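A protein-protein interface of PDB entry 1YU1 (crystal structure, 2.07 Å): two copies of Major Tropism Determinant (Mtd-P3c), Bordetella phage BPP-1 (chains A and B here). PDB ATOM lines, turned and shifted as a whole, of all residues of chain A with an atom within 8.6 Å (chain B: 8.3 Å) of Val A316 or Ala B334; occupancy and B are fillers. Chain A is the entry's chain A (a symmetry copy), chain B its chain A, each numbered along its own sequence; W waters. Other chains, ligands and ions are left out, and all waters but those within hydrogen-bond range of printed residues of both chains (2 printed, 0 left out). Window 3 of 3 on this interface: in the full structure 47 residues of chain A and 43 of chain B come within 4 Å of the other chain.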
ATOM      1  N   PHE A 313     -21.479  -2.571 -33.554  1.00  0.00           N
ATOM      2  CA  PHE A 313     -20.836  -2.661 -32.249  1.00  0.00           C
ATOM      3  C   PHE A 313     -19.526  -1.877 -32.220  1.00  0.00           C
ATOM      4  O   PHE A 313     -18.815  -1.802 -33.216  1.00  0.00           O
ATOM      5  CB  PHE A 313     -20.566  -4.124 -31.886  1.00  0.00           C
ATOM      6  CG  PHE A 313     -21.810  -4.931 -31.675  1.00  0.00           C
ATOM      7  CD1 PHE A 313     -22.372  -5.043 -30.410  1.00  0.00           C
ATOM      8  CD2 PHE A 313     -22.417  -5.585 -32.741  1.00  0.00           C
ATOM      9  CE1 PHE A 313     -23.526  -5.788 -30.210  1.00  0.00           C
ATOM     10  CE2 PHE A 313     -23.573  -6.332 -32.550  1.00  0.00           C
ATOM     11  CZ  PHE A 313     -24.131  -6.431 -31.281  1.00  0.00           C
ATOM     12  N   GLY A 314     -19.210  -1.328 -31.050  1.00  0.00           N
ATOM     13  CA  GLY A 314     -18.064  -0.456 -30.858  1.00  0.00           C
ATOM     14  C   GLY A 314     -18.265   0.442 -29.653  1.00  0.00           C
ATOM     15  O   GLY A 314     -19.360   0.487 -29.076  1.00  0.00           O
ATOM     16  N   GLY A 315     -17.219   1.174 -29.283  1.00  0.00           N
ATOM     17  CA  GLY A 315     -17.249   2.040 -28.113  1.00  0.00           C
ATOM     18  C   GLY A 315     -16.746   1.335 -26.863  1.00  0.00           C
ATOM     19  O   GLY A 315     -15.827   0.521 -26.926  1.00  0.00           O
ATOM     20  N   VAL A 316     -17.363   1.638 -25.729  1.00  0.00           N
ATOM     21  CA  VAL A 316     -16.942   1.094 -24.441  1.00  0.00           C
ATOM     22  C   VAL A 316     -17.266  -0.402 -24.347  1.00  0.00           C
ATOM     23  O   VAL A 316     -18.364  -0.833 -24.687  1.00  0.00           O
ATOM     24  CB  VAL A 316     -17.591   1.869 -23.272  1.00  0.00           C
ATOM     25  CG1 VAL A 316     -17.208   1.254 -21.918  1.00  0.00           C
ATOM     26  CG2 VAL A 316     -17.177   3.343 -23.333  1.00  0.00           C
ATOM     27  N   ASN A 317     -16.292  -1.174 -23.880  1.00  0.00           N
ATOM     28  CA  ASN A 317     -16.404  -2.626 -23.763  1.00  0.00           C
ATOM     29  C   ASN A 317     -16.797  -3.060 -22.361  1.00  0.00           C
ATOM     30  O   ASN A 317     -16.485  -2.385 -21.389  1.00  0.00           O
ATOM     31  CB  ASN A 317     -15.062  -3.284 -24.092  1.00  0.00           C
ATOM     32  CG  ASN A 317     -14.565  -2.942 -25.479  1.00  0.00           C
ATOM     33  OD1 ASN A 317     -15.347  -2.826 -26.422  1.00  0.00           O
ATOM     34  ND2 ASN A 317     -13.253  -2.803 -25.618  1.00  0.00           N
ATOM     35  N   GLY A 318     -17.461  -4.208 -22.262  1.00  0.00           N
ATOM     36  CA  GLY A 318     -17.671  -4.855 -20.983  1.00  0.00           C
ATOM     37  C   GLY A 318     -16.378  -5.509 -20.519  1.00  0.00           C
ATOM     38  O   GLY A 318     -15.337  -5.403 -21.179  1.00  0.00           O
ATOM     39  N   ALA A 319     -16.449  -6.195 -19.386  1.00  0.00           N
ATOM     40  CA  ALA A 319     -15.277  -6.791 -18.762  1.00  0.00           C
ATOM     41  C   ALA A 319     -14.608  -7.818 -19.664  1.00  0.00           C
ATOM     42  O   ALA A 319     -15.273  -8.484 -20.459  1.00  0.00           O
ATOM     43  CB  ALA A 319     -15.662  -7.444 -17.429  1.00  0.00           C
ATOM     44  N   ALA A 334     -15.125  -9.198 -23.321  1.00  0.00           N
ATOM     45  CA  ALA A 334     -14.753  -7.884 -23.847  1.00  0.00           C
ATOM     46  C   ALA A 334     -15.808  -7.354 -24.822  1.00  0.00           C
ATOM     47  O   ALA A 334     -15.477  -6.812 -25.874  1.00  0.00           O
ATOM     48  CB  ALA A 334     -13.378  -7.945 -24.517  1.00  0.00           C
ATOM     49  N   GLN A 335     -17.075  -7.510 -24.452  1.00  0.00           N
ATOM     50  CA  GLN A 335     -18.199  -7.244 -25.347  1.00  0.00           C
ATOM     51  C   GLN A 335     -18.319  -5.750 -25.648  1.00  0.00           C
ATOM     52  O   GLN A 335     -18.576  -4.967 -24.740  1.00  0.00           O
ATOM     53  CB  GLN A 335     -19.501  -7.742 -24.704  1.00  0.00           C
ATOM     54  CG  GLN A 335     -20.786  -7.398 -25.460  1.00  0.00           C
ATOM     55  CD  GLN A 335     -20.829  -7.982 -26.847  1.00  0.00           C
ATOM     56  OE1 GLN A 335     -20.710  -9.198 -27.018  1.00  0.00           O
ATOM     57  NE2 GLN A 335     -21.011  -7.124 -27.848  1.00  0.00           N
ATOM     58  N   PRO A 336     -18.155  -5.342 -26.903  1.00  0.00           N
ATOM     59  CA  PRO A 336     -18.384  -3.937 -27.254  1.00  0.00           C
ATOM     60  C   PRO A 336     -19.848  -3.563 -27.076  1.00  0.00           C
ATOM     61  O   PRO A 336     -20.730  -4.412 -27.230  1.00  0.00           O
ATOM     62  CB  PRO A 336     -17.975  -3.862 -28.724  1.00  0.00           C
ATOM     63  CG  PRO A 336     -18.129  -5.254 -29.235  1.00  0.00           C
ATOM     64  CD  PRO A 336     -17.759  -6.139 -28.078  1.00  0.00           C
ATOM     65  N   ALA A 337     -20.093  -2.300 -26.743  1.00  0.00           N
ATOM     66  CA  ALA A 337     -21.441  -1.756 -26.719  1.00  0.00           C
ATOM     67  C   ALA A 337     -22.091  -1.946 -28.084  1.00  0.00           C
ATOM     68  O   ALA A 337     -21.404  -1.968 -29.111  1.00  0.00           O
ATOM     69  CB  ALA A 337     -21.419  -0.279 -26.364  1.00  0.00           C
ATOM     70  N   ALA A 338     -23.413  -2.110 -28.077  1.00  0.00           N
ATOM     71  CA  ALA A 338     -24.211  -2.038 -29.294  1.00  0.00           C
ATOM     72  C   ALA A 338     -24.592  -0.574 -29.500  1.00  0.00           C
ATOM     73  O   ALA A 338     -24.934   0.130 -28.544  1.00  0.00           O
ATOM     74  CB  ALA A 338     -25.464  -2.901 -29.166  1.00  0.00           C
ATOM     75  N   ALA A 356     -25.583   9.375 -31.512  1.00  0.00           N
ATOM     76  CA  ALA A 356     -25.025   8.035 -31.386  1.00  0.00           C
ATOM     77  C   ALA A 356     -24.361   7.835 -30.022  1.00  0.00           C
ATOM     78  O   ALA A 356     -23.435   8.556 -29.655  1.00  0.00           O
ATOM     79  CB  ALA A 356     -24.028   7.777 -32.513  1.00  0.00           C
ATOM     80  N   LEU A 357     -24.855   6.857 -29.275  1.00  0.00           N
ATOM     81  CA  LEU A 357     -24.338   6.515 -27.960  1.00  0.00           C
ATOM     82  C   LEU A 357     -23.766   5.096 -28.018  1.00  0.00           C
ATOM     83  O   LEU A 357     -24.472   4.157 -28.386  1.00  0.00           O
ATOM     84  CB  LEU A 357     -25.473   6.609 -26.933  1.00  0.00           C
ATOM     85  CG  LEU A 357     -25.264   5.940 -25.577  1.00  0.00           C
ATOM     86  CD1 LEU A 357     -24.084   6.572 -24.872  1.00  0.00           C
ATOM     87  CD2 LEU A 357     -26.526   6.066 -24.750  1.00  0.00           C
ATOM     88  N   TRP A 358     -22.492   4.955 -27.653  1.00  0.00           N
ATOM     89  CA  TRP A 358     -21.764   3.697 -27.782  1.00  0.00           C
ATOM     90  C   TRP A 358     -21.235   3.241 -26.425  1.00  0.00           C
ATOM     91  O   TRP A 358     -20.042   3.031 -26.249  1.00  0.00           O
ATOM     92  CB  TRP A 358     -20.596   3.862 -28.758  1.00  0.00           C
ATOM     93  CG  TRP A 358     -20.960   4.321 -30.139  1.00  0.00           C
ATOM     94  CD1 TRP A 358     -21.197   5.609 -30.541  1.00  0.00           C
ATOM     95  CD2 TRP A 358     -21.074   3.507 -31.317  1.00  0.00           C
ATOM     96  NE1 TRP A 358     -21.462   5.639 -31.890  1.00  0.00           N
ATOM     97  CE2 TRP A 358     -21.394   4.364 -32.392  1.00  0.00           C
ATOM     98  CE3 TRP A 358     -20.935   2.136 -31.577  1.00  0.00           C
ATOM     99  CZ2 TRP A 358     -21.578   3.900 -33.695  1.00  0.00           C
ATOM    100  CZ3 TRP A 358     -21.126   1.671 -32.873  1.00  0.00           C
ATOM    101  CH2 TRP A 358     -21.444   2.552 -33.915  1.00  0.00           C
ATOM    102  N   TYR A 359     -22.137   3.109 -25.461  1.00  0.00           N
ATOM    103  CA  TYR A 359     -21.767   2.792 -24.085  1.00  0.00           C
ATOM    104  C   TYR A 359     -22.516   1.574 -23.531  1.00  0.00           C
ATOM    105  O   TYR A 359     -21.981   0.827 -22.710  1.00  0.00           O
ATOM    106  CB  TYR A 359     -22.033   4.027 -23.216  1.00  0.00           C
ATOM    107  CG  TYR A 359     -21.697   3.851 -21.762  1.00  0.00           C
ATOM    108  CD1 TYR A 359     -20.381   3.943 -21.320  1.00  0.00           C
ATOM    109  CD2 TYR A 359     -22.694   3.587 -20.825  1.00  0.00           C
ATOM    110  CE1 TYR A 359     -20.060   3.774 -19.974  1.00  0.00           C
ATOM    111  CE2 TYR A 359     -22.384   3.415 -19.474  1.00  0.00           C
ATOM    112  CZ  TYR A 359     -21.065   3.511 -19.056  1.00  0.00           C
ATOM    113  OH  TYR A 359     -20.744   3.350 -17.721  1.00  0.00           O
ATOM    114  N   VAL A 360     -23.752   1.379 -23.982  1.00  0.00           N
ATOM    115  CA  VAL A 360     -24.629   0.343 -23.445  1.00  0.00           C
ATOM    116  C   VAL A 360     -24.400  -1.028 -24.095  1.00  0.00           C
ATOM    117  O   VAL A 360     -24.557  -1.190 -25.308  1.00  0.00           O
ATOM    118  CB  VAL A 360     -26.117   0.754 -23.602  1.00  0.00           C
ATOM    119  CG1 VAL A 360     -27.025  -0.259 -22.931  1.00  0.00           C
ATOM    120  CG2 VAL A 360     -26.351   2.156 -23.025  1.00  0.00           C
ATOM    121  N   GLY A 361     -24.047  -2.015 -23.268  1.00  0.00           N
ATOM    122  CA  GLY A 361     -23.914  -3.388 -23.719  1.00  0.00           C
ATOM    123  C   GLY A 361     -25.244  -3.958 -24.191  1.00  0.00           C
ATOM    124  O   GLY A 361     -26.301  -3.505 -23.745  1.00  0.00           O
ATOM    125  N   PRO A 362     -25.198  -4.942 -25.092  1.00  0.00           N
ATOM    126  CA  PRO A 362     -26.414  -5.522 -25.678  1.00  0.00           C
ATOM    127  C   PRO A 362     -27.319  -6.268 -24.683  1.00  0.00           C
ATOM    128  O   PRO A 362     -28.492  -6.491 -24.997  1.00  0.00           O
ATOM    129  CB  PRO A 362     -25.865  -6.486 -26.743  1.00  0.00           C
ATOM    130  CG  PRO A 362     -24.481  -6.789 -26.334  1.00  0.00           C
ATOM    131  CD  PRO A 362     -23.977  -5.565 -25.635  1.00  0.00           C
ATOM    132  N   GLY B 315     -11.958   0.450 -32.844  1.00  0.00           N
ATOM    133  CA  GLY B 315     -10.667   1.050 -32.541  1.00  0.00           C
ATOM    134  C   GLY B 315     -10.764   2.095 -31.441  1.00  0.00           C
ATOM    135  O   GLY B 315     -11.541   1.950 -30.500  1.00  0.00           O
ATOM    136  N   VAL B 316      -9.982   3.159 -31.572  1.00  0.00           N
ATOM    137  CA  VAL B 316      -9.916   4.209 -30.558  1.00  0.00           C
ATOM    138  C   VAL B 316     -11.212   5.026 -30.533  1.00  0.00           C
ATOM    139  O   VAL B 316     -11.727   5.429 -31.573  1.00  0.00           O
ATOM    140  CB  VAL B 316      -8.694   5.127 -30.790  1.00  0.00           C
ATOM    141  CG1 VAL B 316      -8.661   6.275 -29.770  1.00  0.00           C
ATOM    142  CG2 VAL B 316      -7.404   4.302 -30.718  1.00  0.00           C
ATOM    143  N   ASN B 317     -11.721   5.261 -29.329  1.00  0.00           N
ATOM    144  CA  ASN B 317     -12.973   5.983 -29.113  1.00  0.00           C
ATOM    145  C   ASN B 317     -12.742   7.451 -28.797  1.00  0.00           C
ATOM    146  O   ASN B 317     -11.715   7.814 -28.236  1.00  0.00           O
ATOM    147  CB  ASN B 317     -13.736   5.371 -27.936  1.00  0.00           C
ATOM    148  CG  ASN B 317     -14.045   3.903 -28.137  1.00  0.00           C
ATOM    149  OD1 ASN B 317     -14.339   3.464 -29.248  1.00  0.00           O
ATOM    150  ND2 ASN B 317     -14.008   3.140 -27.053  1.00  0.00           N
ATOM    151  N   GLY B 318     -13.716   8.290 -29.136  1.00  0.00           N
ATOM    152  CA  GLY B 318     -13.734   9.662 -28.668  1.00  0.00           C
ATOM    153  C   GLY B 318     -14.144   9.700 -27.204  1.00  0.00           C
ATOM    154  O   GLY B 318     -14.359   8.658 -26.573  1.00  0.00           O
ATOM    155  N   ALA B 319     -14.263  10.908 -26.667  1.00  0.00           N
ATOM    156  CA  ALA B 319     -14.549  11.106 -25.254  1.00  0.00           C
ATOM    157  C   ALA B 319     -15.881  10.493 -24.847  1.00  0.00           C
ATOM    158  O   ALA B 319     -16.815  10.428 -25.649  1.00  0.00           O
ATOM    159  CB  ALA B 319     -14.544  12.602 -24.919  1.00  0.00           C
ATOM    160  N   SER B 320     -15.950  10.061 -23.591  1.00  0.00           N
ATOM    161  CA  SER B 320     -17.188   9.602 -22.974  1.00  0.00           C
ATOM    162  C   SER B 320     -17.973  10.792 -22.404  1.00  0.00           C
ATOM    163  O   SER B 320     -18.172  10.913 -21.190  1.00  0.00           O
ATOM    164  CB  SER B 320     -16.883   8.560 -21.895  1.00  0.00           C
ATOM    165  OG  SER B 320     -16.508   7.332 -22.493  1.00  0.00           O
ATOM    166  N   GLU B 321     -18.398  11.669 -23.311  1.00  0.00           N
ATOM    167  CA  GLU B 321     -19.262  12.809 -23.007  1.00  0.00           C
ATOM    168  C   GLU B 321     -19.997  13.200 -24.284  1.00  0.00           C
ATOM    169  O   GLU B 321     -19.459  13.056 -25.385  1.00  0.00           O
ATOM    170  CB  GLU B 321     -18.444  13.991 -22.475  1.00  0.00           C
ATOM    171  CG  GLU B 321     -17.509  14.640 -23.495  1.00  0.00           C
ATOM    172  CD  GLU B 321     -16.548  15.638 -22.867  1.00  0.00           C
ATOM    173  OE1 GLU B 321     -16.785  16.052 -21.714  1.00  0.00           O
ATOM    174  OE2 GLU B 321     -15.546  16.013 -23.525  1.00  0.00           O
ATOM    175  N   TYR B 322     -21.224  13.688 -24.152  1.00  0.00           N
ATOM    176  CA  TYR B 322     -22.004  14.053 -25.333  1.00  0.00           C
ATOM    177  C   TYR B 322     -21.300  15.182 -26.090  1.00  0.00           C
ATOM    178  O   TYR B 322     -21.061  16.256 -25.534  1.00  0.00           O
ATOM    179  CB  TYR B 322     -23.444  14.421 -24.960  1.00  0.00           C
ATOM    180  CG  TYR B 322     -24.306  13.204 -24.710  1.00  0.00           C
ATOM    181  CD1 TYR B 322     -24.649  12.352 -25.759  1.00  0.00           C
ATOM    182  CD2 TYR B 322     -24.753  12.885 -23.432  1.00  0.00           C
ATOM    183  CE1 TYR B 322     -25.424  11.224 -25.548  1.00  0.00           C
ATOM    184  CE2 TYR B 322     -25.535  11.743 -23.207  1.00  0.00           C
ATOM    185  CZ  TYR B 322     -25.862  10.925 -24.277  1.00  0.00           C
ATOM    186  OH  TYR B 322     -26.622   9.801 -24.085  1.00  0.00           O
ATOM    187  N   THR B 323     -20.954  14.905 -27.350  1.00  0.00           N
ATOM    188  CA  THR B 323     -20.111  15.775 -28.159  1.00  0.00           C
ATOM    189  C   THR B 323     -20.811  16.131 -29.472  1.00  0.00           C
ATOM    190  O   THR B 323     -21.057  15.261 -30.309  1.00  0.00           O
ATOM    191  CB  THR B 323     -18.773  15.072 -28.450  1.00  0.00           C
ATOM    192  OG1 THR B 323     -18.123  14.748 -27.215  1.00  0.00           O
ATOM    193  CG2 THR B 323     -17.793  16.006 -29.164  1.00  0.00           C
ATOM    194  N   SER B 331     -25.468  14.753 -30.971  1.00  0.00           N
ATOM    195  CA  SER B 331     -24.184  14.504 -30.331  1.00  0.00           C
ATOM    196  C   SER B 331     -23.866  13.014 -30.259  1.00  0.00           C
ATOM    197  O   SER B 331     -24.763  12.176 -30.285  1.00  0.00           O
ATOM    198  CB  SER B 331     -24.192  15.085 -28.918  1.00  0.00           C
ATOM    199  OG  SER B 331     -24.466  16.476 -28.951  1.00  0.00           O
ATOM    200  N   VAL B 332     -22.577  12.709 -30.159  1.00  0.00           N
ATOM    201  CA  VAL B 332     -22.098  11.336 -30.010  1.00  0.00           C
ATOM    202  C   VAL B 332     -21.410  11.153 -28.660  1.00  0.00           C
ATOM    203  O   VAL B 332     -20.978  12.116 -28.039  1.00  0.00           O
ATOM    204  CB  VAL B 332     -21.148  10.922 -31.164  1.00  0.00           C
ATOM    205  CG1 VAL B 332     -21.812  11.164 -32.510  1.00  0.00           C
ATOM    206  CG2 VAL B 332     -19.804  11.645 -31.079  1.00  0.00           C
ATOM    207  N   TYR B 333     -21.303   9.903 -28.222  1.00  0.00           N
ATOM    208  CA  TYR B 333     -20.791   9.580 -26.897  1.00  0.00           C
ATOM    209  C   TYR B 333     -19.975   8.296 -26.995  1.00  0.00           C
ATOM    210  O   TYR B 333     -20.487   7.268 -27.431  1.00  0.00           O
ATOM    211  CB  TYR B 333     -21.955   9.415 -25.915  1.00  0.00           C
ATOM    212  CG  TYR B 333     -21.554   9.294 -24.461  1.00  0.00           C
ATOM    213  CD1 TYR B 333     -21.811  10.330 -23.558  1.00  0.00           C
ATOM    214  CD2 TYR B 333     -20.930   8.141 -23.978  1.00  0.00           C
ATOM    215  CE1 TYR B 333     -21.460  10.218 -22.216  1.00  0.00           C
ATOM    216  CE2 TYR B 333     -20.578   8.023 -22.640  1.00  0.00           C
ATOM    217  CZ  TYR B 333     -20.842   9.063 -21.763  1.00  0.00           C
ATOM    218  OH  TYR B 333     -20.483   8.951 -20.435  1.00  0.00           O
ATOM    219  N   ALA B 334     -18.712   8.367 -26.582  1.00  0.00           N
ATOM    220  CA  ALA B 334     -17.769   7.256 -26.713  1.00  0.00           C
ATOM    221  C   ALA B 334     -17.698   6.750 -28.157  1.00  0.00           C
ATOM    222  O   ALA B 334     -17.679   5.547 -28.402  1.00  0.00           O
ATOM    223  CB  ALA B 334     -18.145   6.120 -25.759  1.00  0.00           C
ATOM    224  N   GLN B 335     -17.651   7.685 -29.101  1.00  0.00           N
ATOM    225  CA  GLN B 335     -17.781   7.380 -30.524  1.00  0.00           C
ATOM    226  C   GLN B 335     -16.567   6.601 -31.031  1.00  0.00           C
ATOM    227  O   GLN B 335     -15.461   7.129 -31.024  1.00  0.00           O
ATOM    228  CB  GLN B 335     -17.921   8.683 -31.322  1.00  0.00           C
ATOM    229  CG  GLN B 335     -17.917   8.532 -32.844  1.00  0.00           C
ATOM    230  CD  GLN B 335     -19.048   7.680 -33.355  1.00  0.00           C
ATOM    231  OE1 GLN B 335     -20.219   7.974 -33.097  1.00  0.00           O
ATOM    232  NE2 GLN B 335     -18.712   6.624 -34.092  1.00  0.00           N
ATOM    233  N   PRO B 336     -16.754   5.363 -31.484  1.00  0.00           N
ATOM    234  CA  PRO B 336     -15.640   4.630 -32.094  1.00  0.00           C
ATOM    235  C   PRO B 336     -15.197   5.291 -33.390  1.00  0.00           C
ATOM    236  O   PRO B 336     -16.010   5.909 -34.083  1.00  0.00           O
ATOM    237  CB  PRO B 336     -16.225   3.244 -32.358  1.00  0.00           C
ATOM    238  CG  PRO B 336     -17.696   3.461 -32.453  1.00  0.00           C
ATOM    239  CD  PRO B 336     -17.992   4.566 -31.477  1.00  0.00           C
ATOM    240  N   ALA B 337     -13.911   5.165 -33.701  1.00  0.00           N
ATOM    241  CA  ALA B 337     -13.384   5.583 -34.991  1.00  0.00           C
ATOM    242  C   ALA B 337     -14.140   4.869 -36.104  1.00  0.00           C
ATOM    243  O   ALA B 337     -14.623   3.747 -35.918  1.00  0.00           O
ATOM    244  CB  ALA B 337     -11.901   5.268 -35.093  1.00  0.00           C
HETATM  245  O   HOH W   1     -14.423   0.755 -30.066  1.00  0.00           O
HETATM  246  O   HOH W   2     -13.212   0.441 -26.256  1.00  0.00           O
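The backbone carbonyl oxygen of Gly A315 sits at hydrogen-bond distance from the side-chain amide nitrogen of Asn B317, 3.2 Å away. The backbone carbonyl oxygen (O) of Ser B331 lies within hydrogen-bond range of the backbone NH (N) of Ala A356. The backbone carbonyl oxygen of Ala A356 sits at hydrogen-bond distance from the backbone NH of Tyr B333, at 2.9 Å. The backbone carbonyl oxygen of Tyr B333 is in hydrogen-bond range of the backbone NH of Trp A358, 3.1 Å away. The side-chain amide oxygen (OE1) of Gln B335 is in hydrogen-bond range of the indole nitrogen (NE1) of Trp A358 (2.9 Å).
O of Gly B315 lies close to OD1 of Asn B317. The backbone NH (N) of Gly B318 is in hydrogen-bond range of the backbone carbonyl oxygen (O) of Gln B335 (2.8 Å). N of Thr B323 is in hydrogen-bond range of O of Val B332. O of Gly A315 sits close to OD1 of Asn A317 (3.4 Å). O of Val A316 is in hydrogen-bond range of N of Ala A337. O of Trp A358 sits at hydrogen-bond distance from N of Val A316 (3.1 Å).
Among the printed residues, pairs that only touch across the chains: Gly A315 with Ala B334 (3.5 Å), Gly A315 with Pro B336 (3.8 Å), Val A316 with Asn B317 (3.9 Å), Val A316 with Ala B334 (3.8 Å), Ala A356 with Val B332 (3.1 Å), Ala A356 with Gln B335 (3.9 Å), Leu A357 with Tyr B322 (3.8 Å), Leu A357 with Tyr B333 (3.6 Å), Trp A358 with Ala B334 (3.4 Å) and Trp A358 with Pro B336 (3.3 Å).
Gly A315 touches three residues of chain B. Val A316 touches two residues of chain B. Ala A319 touches none of the printed residues of chain B. Of the printed residues of chain B, Ala A356 touches Ser B331 (3.2 Å), Val B332 (3.1 Å), Tyr B333 (2.9 Å) and Gln B335 (3.9 Å). Of the printed residues of chain B, Leu A357 touches Tyr B322 and Tyr B333. Printed residues of chain A within 4 Å of Asn B317: Gly A315 and Val A316. Of the printed residues of chain A, Ala B334 touches Gly A315 (3.5 Å), Val A316 (3.8 Å) and Trp A358 (3.4 Å). Of the printed residues of chain A, Gln B335 touches Ala A356 and Trp A358. The nearest residue of chain B that does not touch Val A316 is Ser B320 (4.1 Å). The nearest residue of chain A that does not touch Ala B334 is Tyr A359 (5.0 Å).
Of the 19 printed residues of chain A, 5 touch a printed residue of chain B. Printed residues of chain A that touch a printed residue of chain B: Gly A315, Val A316, Ala A356, Leu A357 and Trp A358. Along chain A the printed residues that touch a printed residue of chain B span positions 315 to 358. Of the 16 printed residues of chain B, 8 touch a printed residue of chain A. Printed residues of chain B that touch a printed residue of chain A: Asn B317, Tyr B322, Ser B331, Val B332, Tyr B333, Ala B334, Gln B335 and Pro B336. Among the printed residues, no Asp or Glu carboxylate lies within 4 Å of a Lys or Arg side-chain nitrogen of the other chain.
Gly A315 touches Asn B317, but with the chains exchanged Asn A317 does not touch Gly B315 (7.0 Å). Gly A315 touches Pro B336, but with the chains exchanged Pro A336 does not touch Gly B315 (8.5 Å). Val A316 touches Asn B317, but with the chains exchanged Asn A317 does not touch Val B316 (9.0 Å). Val A316 touches Ala B334, but with the chains exchanged Ala A334 does not touch Val B316 (12.7 Å). Of the 15 pairs that touch across the chains among the printed residues, none has its exchanged pair printed and touching as well.
Water W2 lies within hydrogen-bond range of the backbone carbonyl oxygen (O) of Gly A315, the side-chain amide nitrogen (ND2) of Asn B317 and the side-chain amide nitrogen (ND2) of Asn A317. Water W1 lies within hydrogen-bond range of OD1 of Asn B317, N of Gly A315 and O of Gly B315.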
